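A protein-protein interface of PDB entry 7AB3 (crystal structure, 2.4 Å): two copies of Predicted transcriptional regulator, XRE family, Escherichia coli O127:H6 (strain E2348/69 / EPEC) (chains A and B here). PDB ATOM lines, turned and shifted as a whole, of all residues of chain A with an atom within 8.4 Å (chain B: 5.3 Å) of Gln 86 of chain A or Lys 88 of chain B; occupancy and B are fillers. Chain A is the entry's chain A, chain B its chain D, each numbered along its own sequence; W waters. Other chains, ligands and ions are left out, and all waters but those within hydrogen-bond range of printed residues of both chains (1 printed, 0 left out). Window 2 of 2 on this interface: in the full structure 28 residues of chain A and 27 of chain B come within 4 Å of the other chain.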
ATOM      1  N   PRO A  45     -18.095 -26.090 -27.385  1.00  0.00           N
ATOM      2  CA  PRO A  45     -19.253 -26.166 -26.470  1.00  0.00           C
ATOM      3  C   PRO A  45     -20.619 -26.085 -27.199  1.00  0.00           C
ATOM      4  O   PRO A  45     -21.543 -26.843 -26.900  1.00  0.00           O
ATOM      5  CB  PRO A  45     -19.021 -24.970 -25.535  1.00  0.00           C
ATOM      6  CG  PRO A  45     -17.528 -24.791 -25.539  1.00  0.00           C
ATOM      7  CD  PRO A  45     -17.146 -25.039 -26.962  1.00  0.00           C
ATOM      8  N   THR A  76     -31.795 -20.989 -18.303  1.00  0.00           N
ATOM      9  CA  THR A  76     -30.448 -21.560 -18.324  1.00  0.00           C
ATOM     10  C   THR A  76     -30.432 -22.718 -19.324  1.00  0.00           C
ATOM     11  O   THR A  76     -29.471 -22.842 -20.075  1.00  0.00           O
ATOM     12  CB  THR A  76     -29.998 -22.022 -16.929  1.00  0.00           C
ATOM     13  OG1 THR A  76     -29.919 -20.902 -16.068  1.00  0.00           O
ATOM     14  CG2 THR A  76     -28.655 -22.683 -16.939  1.00  0.00           C
ATOM     15  N   ARG A  79     -30.041 -21.328 -22.767  1.00  0.00           N
ATOM     16  CA  ARG A  79     -28.670 -20.886 -22.995  1.00  0.00           C
ATOM     17  C   ARG A  79     -27.790 -22.102 -23.246  1.00  0.00           C
ATOM     18  O   ARG A  79     -26.988 -22.076 -24.158  1.00  0.00           O
ATOM     19  CB  ARG A  79     -28.140 -20.096 -21.787  1.00  0.00           C
ATOM     20  CG  ARG A  79     -29.007 -18.909 -21.363  1.00  0.00           C
ATOM     21  CD  ARG A  79     -28.351 -18.010 -20.310  1.00  0.00           C
ATOM     22  NE  ARG A  79     -27.997 -18.703 -19.066  1.00  0.00           N
ATOM     23  CZ  ARG A  79     -26.762 -19.087 -18.745  1.00  0.00           C
ATOM     24  NH1 ARG A  79     -26.531 -19.702 -17.590  1.00  0.00           N
ATOM     25  NH2 ARG A  79     -25.748 -18.850 -19.570  1.00  0.00           N
ATOM     26  N   LEU A  80     -27.967 -23.174 -22.460  1.00  0.00           N
ATOM     27  CA  LEU A  80     -27.274 -24.450 -22.525  1.00  0.00           C
ATOM     28  C   LEU A  80     -27.419 -25.086 -23.918  1.00  0.00           C
ATOM     29  O   LEU A  80     -26.432 -25.509 -24.497  1.00  0.00           O
ATOM     30  CB  LEU A  80     -27.889 -25.372 -21.440  1.00  0.00           C
ATOM     31  CG  LEU A  80     -27.137 -26.641 -21.007  1.00  0.00           C
ATOM     32  CD1 LEU A  80     -27.437 -26.968 -19.563  1.00  0.00           C
ATOM     33  CD2 LEU A  80     -27.517 -27.832 -21.855  1.00  0.00           C
ATOM     34  N   ASP A  83     -25.453 -22.593 -26.570  1.00  0.00           N
ATOM     35  CA  ASP A  83     -24.007 -22.567 -26.343  1.00  0.00           C
ATOM     36  C   ASP A  83     -23.769 -22.665 -24.836  1.00  0.00           C
ATOM     37  O   ASP A  83     -23.911 -21.669 -24.118  1.00  0.00           O
ATOM     38  CB  ASP A  83     -23.359 -21.281 -26.911  1.00  0.00           C
ATOM     39  CG  ASP A  83     -21.835 -21.271 -26.869  1.00  0.00           C
ATOM     40  OD1 ASP A  83     -21.243 -22.330 -26.578  1.00  0.00           O
ATOM     41  OD2 ASP A  83     -21.235 -20.199 -27.141  1.00  0.00           O
ATOM     42  N   PRO A  84     -23.415 -23.857 -24.333  1.00  0.00           N
ATOM     43  CA  PRO A  84     -23.198 -24.009 -22.898  1.00  0.00           C
ATOM     44  C   PRO A  84     -21.843 -23.534 -22.389  1.00  0.00           C
ATOM     45  O   PRO A  84     -21.493 -23.848 -21.269  1.00  0.00           O
ATOM     46  CB  PRO A  84     -23.363 -25.500 -22.696  1.00  0.00           C
ATOM     47  CG  PRO A  84     -22.834 -26.063 -23.943  1.00  0.00           C
ATOM     48  CD  PRO A  84     -23.266 -25.138 -25.032  1.00  0.00           C
ATOM     49  N   GLU A  85     -21.110 -22.734 -23.162  1.00  0.00           N
ATOM     50  CA  GLU A  85     -19.841 -22.121 -22.794  1.00  0.00           C
ATOM     51  C   GLU A  85     -19.869 -21.505 -21.375  1.00  0.00           C
ATOM     52  O   GLU A  85     -18.969 -21.760 -20.576  1.00  0.00           O
ATOM     53  CB  GLU A  85     -19.493 -21.042 -23.848  1.00  0.00           C
ATOM     54  CG  GLU A  85     -18.363 -20.082 -23.480  1.00  0.00           C
ATOM     55  CD  GLU A  85     -16.949 -20.595 -23.706  1.00  0.00           C
ATOM     56  OE1 GLU A  85     -16.000 -20.089 -23.054  1.00  0.00           O
ATOM     57  OE2 GLU A  85     -16.795 -21.523 -24.536  1.00  0.00           O
ATOM     58  N   GLN A  86     -20.892 -20.701 -21.086  1.00  0.00           N
ATOM     59  CA  GLN A  86     -21.035 -19.980 -19.822  1.00  0.00           C
ATOM     60  C   GLN A  86     -21.890 -20.672 -18.769  1.00  0.00           C
ATOM     61  O   GLN A  86     -22.029 -20.147 -17.666  1.00  0.00           O
ATOM     62  CB  GLN A  86     -21.569 -18.564 -20.080  1.00  0.00           C
ATOM     63  CG  GLN A  86     -20.780 -17.780 -21.118  1.00  0.00           C
ATOM     64  CD  GLN A  86     -19.404 -17.428 -20.616  1.00  0.00           C
ATOM     65  OE1 GLN A  86     -19.201 -17.207 -19.416  1.00  0.00           O
ATOM     66  NE2 GLN A  86     -18.424 -17.321 -21.515  1.00  0.00           N
ATOM     67  N   VAL A  87     -22.468 -21.829 -19.104  1.00  0.00           N
ATOM     68  CA  VAL A  87     -23.271 -22.648 -18.203  1.00  0.00           C
ATOM     69  C   VAL A  87     -22.321 -23.508 -17.361  1.00  0.00           C
ATOM     70  O   VAL A  87     -21.273 -23.914 -17.866  1.00  0.00           O
ATOM     71  CB  VAL A  87     -24.248 -23.519 -19.032  1.00  0.00           C
ATOM     72  CG1 VAL A  87     -25.083 -24.432 -18.137  1.00  0.00           C
ATOM     73  CG2 VAL A  87     -25.145 -22.637 -19.909  1.00  0.00           C
ATOM     74  N   LYS A  88     -22.660 -23.780 -16.080  1.00  0.00           N
ATOM     75  CA  LYS A  88     -21.794 -24.596 -15.239  1.00  0.00           C
ATOM     76  C   LYS A  88     -21.733 -26.056 -15.754  1.00  0.00           C
ATOM     77  O   LYS A  88     -22.718 -26.560 -16.294  1.00  0.00           O
ATOM     78  CB  LYS A  88     -22.162 -24.466 -13.756  1.00  0.00           C
ATOM     79  CG  LYS A  88     -23.474 -25.068 -13.390  1.00  0.00           C
ATOM     80  CD  LYS A  88     -23.602 -25.283 -11.882  1.00  0.00           C
ATOM     81  CE  LYS A  88     -24.289 -26.595 -11.551  1.00  0.00           C
ATOM     82  NZ  LYS A  88     -24.407 -26.829 -10.080  1.00  0.00           N
ATOM     83  N   PHE A  89     -20.535 -26.684 -15.682  1.00  0.00           N
ATOM     84  CA  PHE A  89     -20.275 -28.029 -16.186  1.00  0.00           C
ATOM     85  C   PHE A  89     -21.270 -29.050 -15.628  1.00  0.00           C
ATOM     86  O   PHE A  89     -21.764 -29.886 -16.387  1.00  0.00           O
ATOM     87  CB  PHE A  89     -18.810 -28.463 -15.951  1.00  0.00           C
ATOM     88  CG  PHE A  89     -18.544 -29.878 -16.418  1.00  0.00           C
ATOM     89  CD1 PHE A  89     -18.358 -30.155 -17.754  1.00  0.00           C
ATOM     90  CD2 PHE A  89     -18.586 -30.939 -15.532  1.00  0.00           C
ATOM     91  CE1 PHE A  89     -18.178 -31.460 -18.191  1.00  0.00           C
ATOM     92  CE2 PHE A  89     -18.441 -32.246 -15.981  1.00  0.00           C
ATOM     93  CZ  PHE A  89     -18.229 -32.494 -17.306  1.00  0.00           C
ATOM     94  N   GLY A  90     -21.556 -28.966 -14.321  1.00  0.00           N
ATOM     95  CA  GLY A  90     -22.499 -29.836 -13.638  1.00  0.00           C
ATOM     96  C   GLY A  90     -23.904 -29.846 -14.205  1.00  0.00           C
ATOM     97  O   GLY A  90     -24.586 -30.862 -14.132  1.00  0.00           O
ATOM     98  N   SER A  91     -24.359 -28.721 -14.759  1.00  0.00           N
ATOM     99  CA  SER A  91     -25.681 -28.595 -15.389  1.00  0.00           C
ATOM    100  C   SER A  91     -25.688 -29.238 -16.767  1.00  0.00           C
ATOM    101  O   SER A  91     -26.648 -29.904 -17.137  1.00  0.00           O
ATOM    102  CB  SER A  91     -26.089 -27.133 -15.492  1.00  0.00           C
ATOM    103  OG  SER A  91     -26.388 -26.633 -14.197  1.00  0.00           O
ATOM    104  N   VAL A  92     -24.615 -29.056 -17.527  1.00  0.00           N
ATOM    105  CA  VAL A  92     -24.446 -29.692 -18.826  1.00  0.00           C
ATOM    106  C   VAL A  92     -24.384 -31.218 -18.618  1.00  0.00           C
ATOM    107  O   VAL A  92     -25.073 -31.951 -19.318  1.00  0.00           O
ATOM    108  CB  VAL A  92     -23.178 -29.160 -19.557  1.00  0.00           C
ATOM    109  CG1 VAL A  92     -22.992 -29.846 -20.907  1.00  0.00           C
ATOM    110  CG2 VAL A  92     -23.235 -27.643 -19.717  1.00  0.00           C
ATOM    111  N   PRO B  84     -15.213 -29.995 -11.103  1.00  0.00           N
ATOM    112  CA  PRO B  84     -15.605 -28.908 -12.000  1.00  0.00           C
ATOM    113  C   PRO B  84     -17.089 -28.597 -12.044  1.00  0.00           C
ATOM    114  O   PRO B  84     -17.468 -27.751 -12.825  1.00  0.00           O
ATOM    115  CB  PRO B  84     -15.112 -29.396 -13.362  1.00  0.00           C
ATOM    116  CG  PRO B  84     -15.198 -30.869 -13.278  1.00  0.00           C
ATOM    117  CD  PRO B  84     -14.826 -31.204 -11.858  1.00  0.00           C
ATOM    118  N   GLN B  86     -19.184 -26.686 -10.504  1.00  0.00           N
ATOM    119  CA  GLN B  86     -19.551 -25.272 -10.502  1.00  0.00           C
ATOM    120  C   GLN B  86     -18.746 -24.376 -11.425  1.00  0.00           C
ATOM    121  O   GLN B  86     -18.994 -23.176 -11.464  1.00  0.00           O
ATOM    122  CB  GLN B  86     -19.494 -24.715  -9.074  1.00  0.00           C
ATOM    123  CG  GLN B  86     -20.296 -25.530  -8.049  1.00  0.00           C
ATOM    124  CD  GLN B  86     -21.792 -25.509  -8.264  1.00  0.00           C
ATOM    125  OE1 GLN B  86     -22.508 -26.423  -7.807  1.00  0.00           O
ATOM    126  NE2 GLN B  86     -22.316 -24.488  -8.957  1.00  0.00           N
ATOM    127  N   VAL B  87     -17.759 -24.938 -12.125  1.00  0.00           N
ATOM    128  CA  VAL B  87     -16.913 -24.253 -13.091  1.00  0.00           C
ATOM    129  C   VAL B  87     -17.672 -24.195 -14.431  1.00  0.00           C
ATOM    130  O   VAL B  87     -18.419 -25.132 -14.742  1.00  0.00           O
ATOM    131  CB  VAL B  87     -15.562 -25.005 -13.234  1.00  0.00           C
ATOM    132  CG1 VAL B  87     -14.665 -24.350 -14.281  1.00  0.00           C
ATOM    133  CG2 VAL B  87     -14.854 -25.106 -11.892  1.00  0.00           C
ATOM    134  N   LYS B  88     -17.498 -23.094 -15.213  1.00  0.00           N
ATOM    135  CA  LYS B  88     -18.191 -22.968 -16.488  1.00  0.00           C
ATOM    136  C   LYS B  88     -17.682 -24.006 -17.496  1.00  0.00           C
ATOM    137  O   LYS B  88     -16.506 -24.358 -17.484  1.00  0.00           O
ATOM    138  CB  LYS B  88     -18.178 -21.533 -17.015  1.00  0.00           C
ATOM    139  CG  LYS B  88     -16.820 -21.033 -17.412  1.00  0.00           C
ATOM    140  CD  LYS B  88     -16.921 -19.792 -18.308  1.00  0.00           C
ATOM    141  CE  LYS B  88     -15.905 -19.816 -19.427  1.00  0.00           C
ATOM    142  NZ  LYS B  88     -15.897 -18.552 -20.212  1.00  0.00           N
ATOM    143  N   PHE B  89     -18.603 -24.578 -18.301  1.00  0.00           N
ATOM    144  CA  PHE B  89     -18.315 -25.633 -19.281  1.00  0.00           C
ATOM    145  C   PHE B  89     -17.177 -25.256 -20.218  1.00  0.00           C
ATOM    146  O   PHE B  89     -16.316 -26.080 -20.473  1.00  0.00           O
ATOM    147  CB  PHE B  89     -19.591 -26.070 -20.060  1.00  0.00           C
ATOM    148  CG  PHE B  89     -19.292 -27.155 -21.075  1.00  0.00           C
ATOM    149  CD1 PHE B  89     -19.144 -28.474 -20.683  1.00  0.00           C
ATOM    150  CD2 PHE B  89     -19.057 -26.845 -22.395  1.00  0.00           C
ATOM    151  CE1 PHE B  89     -18.776 -29.458 -21.599  1.00  0.00           C
ATOM    152  CE2 PHE B  89     -18.676 -27.830 -23.302  1.00  0.00           C
ATOM    153  CZ  PHE B  89     -18.553 -29.130 -22.899  1.00  0.00           C
ATOM    154  N   GLY B  90     -17.178 -24.020 -20.709  1.00  0.00           N
ATOM    155  CA  GLY B  90     -16.149 -23.491 -21.593  1.00  0.00           C
ATOM    156  C   GLY B  90     -14.736 -23.533 -21.050  1.00  0.00           C
ATOM    157  O   GLY B  90     -13.794 -23.685 -21.827  1.00  0.00           O
ATOM    158  N   SER B  91     -14.565 -23.392 -19.732  1.00  0.00           N
ATOM    159  CA  SER B  91     -13.257 -23.470 -19.055  1.00  0.00           C
ATOM    160  C   SER B  91     -12.795 -24.922 -18.938  1.00  0.00           C
ATOM    161  O   SER B  91     -11.624 -25.218 -19.130  1.00  0.00           O
ATOM    162  CB  SER B  91     -13.337 -22.853 -17.664  1.00  0.00           C
ATOM    163  OG  SER B  91     -13.448 -21.445 -17.788  1.00  0.00           O
ATOM    164  N   VAL B  92     -13.713 -25.840 -18.635  1.00  0.00           N
ATOM    165  CA  VAL B  92     -13.424 -27.266 -18.587  1.00  0.00           C
ATOM    166  C   VAL B  92     -13.023 -27.726 -19.989  1.00  0.00           C
ATOM    167  O   VAL B  92     -12.016 -28.404 -20.135  1.00  0.00           O
ATOM    168  CB  VAL B  92     -14.649 -28.069 -18.038  1.00  0.00           C
ATOM    169  CG1 VAL B  92     -14.356 -29.569 -18.009  1.00  0.00           C
ATOM    170  CG2 VAL B  92     -15.053 -27.571 -16.662  1.00  0.00           C
HETATM  171  O   HOH W   1     -14.237 -23.575 -24.625  1.00  0.00           O
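Thr 76 of chain A touches none of the printed residues of chain B. Of the printed residues of chain B, Pro 84 of chain A touches Phe 89. Of the printed residues of chain B, Glu 85 of chain A touches Lys 88 (3.2 Å), Phe 89 (3.6 Å) and Gly 90 (2.9 Å). Printed residues of chain B within 4 Å of Lys 88 of chain A: Gln 86 and Val 87. Ser 91 of chain A touches none of the printed residues of chain B. Lys 88 of chain B touches just these residues of chain A: Glu 85, Gln 86 and Val 87. Of the printed residues of chain A, Gly 90 of chain B touches Glu 85. The nearest residue of chain A that does not touch Lys 88 of chain B is Lys 88 of chain A (4.1 Å). The nearest printed residue of chain A that does not touch Val 92 of chain B is Lys 88 of chain A (6.9 Å).
NZ of Lys 88 of chain B lies within salt-bridge range of OE1 of Glu 85 of chain A (3.2 Å). O of Glu 85 of chain A lies within hydrogen-bond range of N of Gly 90 of chain B (2.9 Å). The side-chain amino group (NZ) of Lys 88 of chain B lies close to the side-chain amide nitrogen (NE2) of Gln 86 of chain A (3.1 Å). The backbone NH of Phe 89 of chain B sits at hydrogen-bond distance from the backbone carbonyl oxygen of Val 87 of chain A. OE1 of Gln 86 of chain B is in hydrogen-bond range of NZ of Lys 88 of chain A (3.0 Å). N of Phe 89 of chain A is in hydrogen-bond range of O of Val 87 of chain B (2.8 Å).
The side-chain carboxylate of Asp 83 of chain A sits close to the backbone NH of Glu 85 of chain A (3.4 Å).
CA of Pro 45 of chain A touches CE2 of Phe 89 of chain B, at 3.6 Å. Pro 84 of chain A touches Phe 89 of chain B. Phe 89 of chain B touches Glu 85 of chain A. Val 87 of chain A touches Lys 88 of chain B. CA of Lys 88 of chain A touches O of Val 87 of chain B, at 3.5 Å. Phe 89 of chain A touches Pro 84 of chain B. Phe 89 of chain B touches Phe 89 of chain A. Val 92 of chain B touches Phe 89 of chain A. Phe 89 of chain B touches Val 92 of chain A.
Water W1 lies within hydrogen-bond range of O of Gly 90 of chain B and OE2 of Glu 85 of chain A.
Of the 14 printed residues of chain A, 8 touch a printed residue of chain B. Hydrophobic or aromatic side chains of chain A that line the printed part of chain B: Pro 45, Phe 89 and Val 92. Hydrophobic or aromatic side chains of chain B within 4 Å of the printed part of chain A: Phe 89 and Val 92.
Gln 86 of chain A touches Lys 88 of chain B, and with the chains exchanged Lys 88 of chain A touches Gln 86 of chain B. Val 87 of chain A touches Lys 88 of chain B, and with the chains exchanged Lys 88 of chain A touches Val 87 of chain B. Val 87 of chain A touches Phe 89 of chain B, and with the chains exchanged Phe 89 of chain A touches Val 87 of chain B. Phe 89 of chain A touches Val 92 of chain B, and with the chains exchanged Val 92 of chain A touches Phe 89 of chain B.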
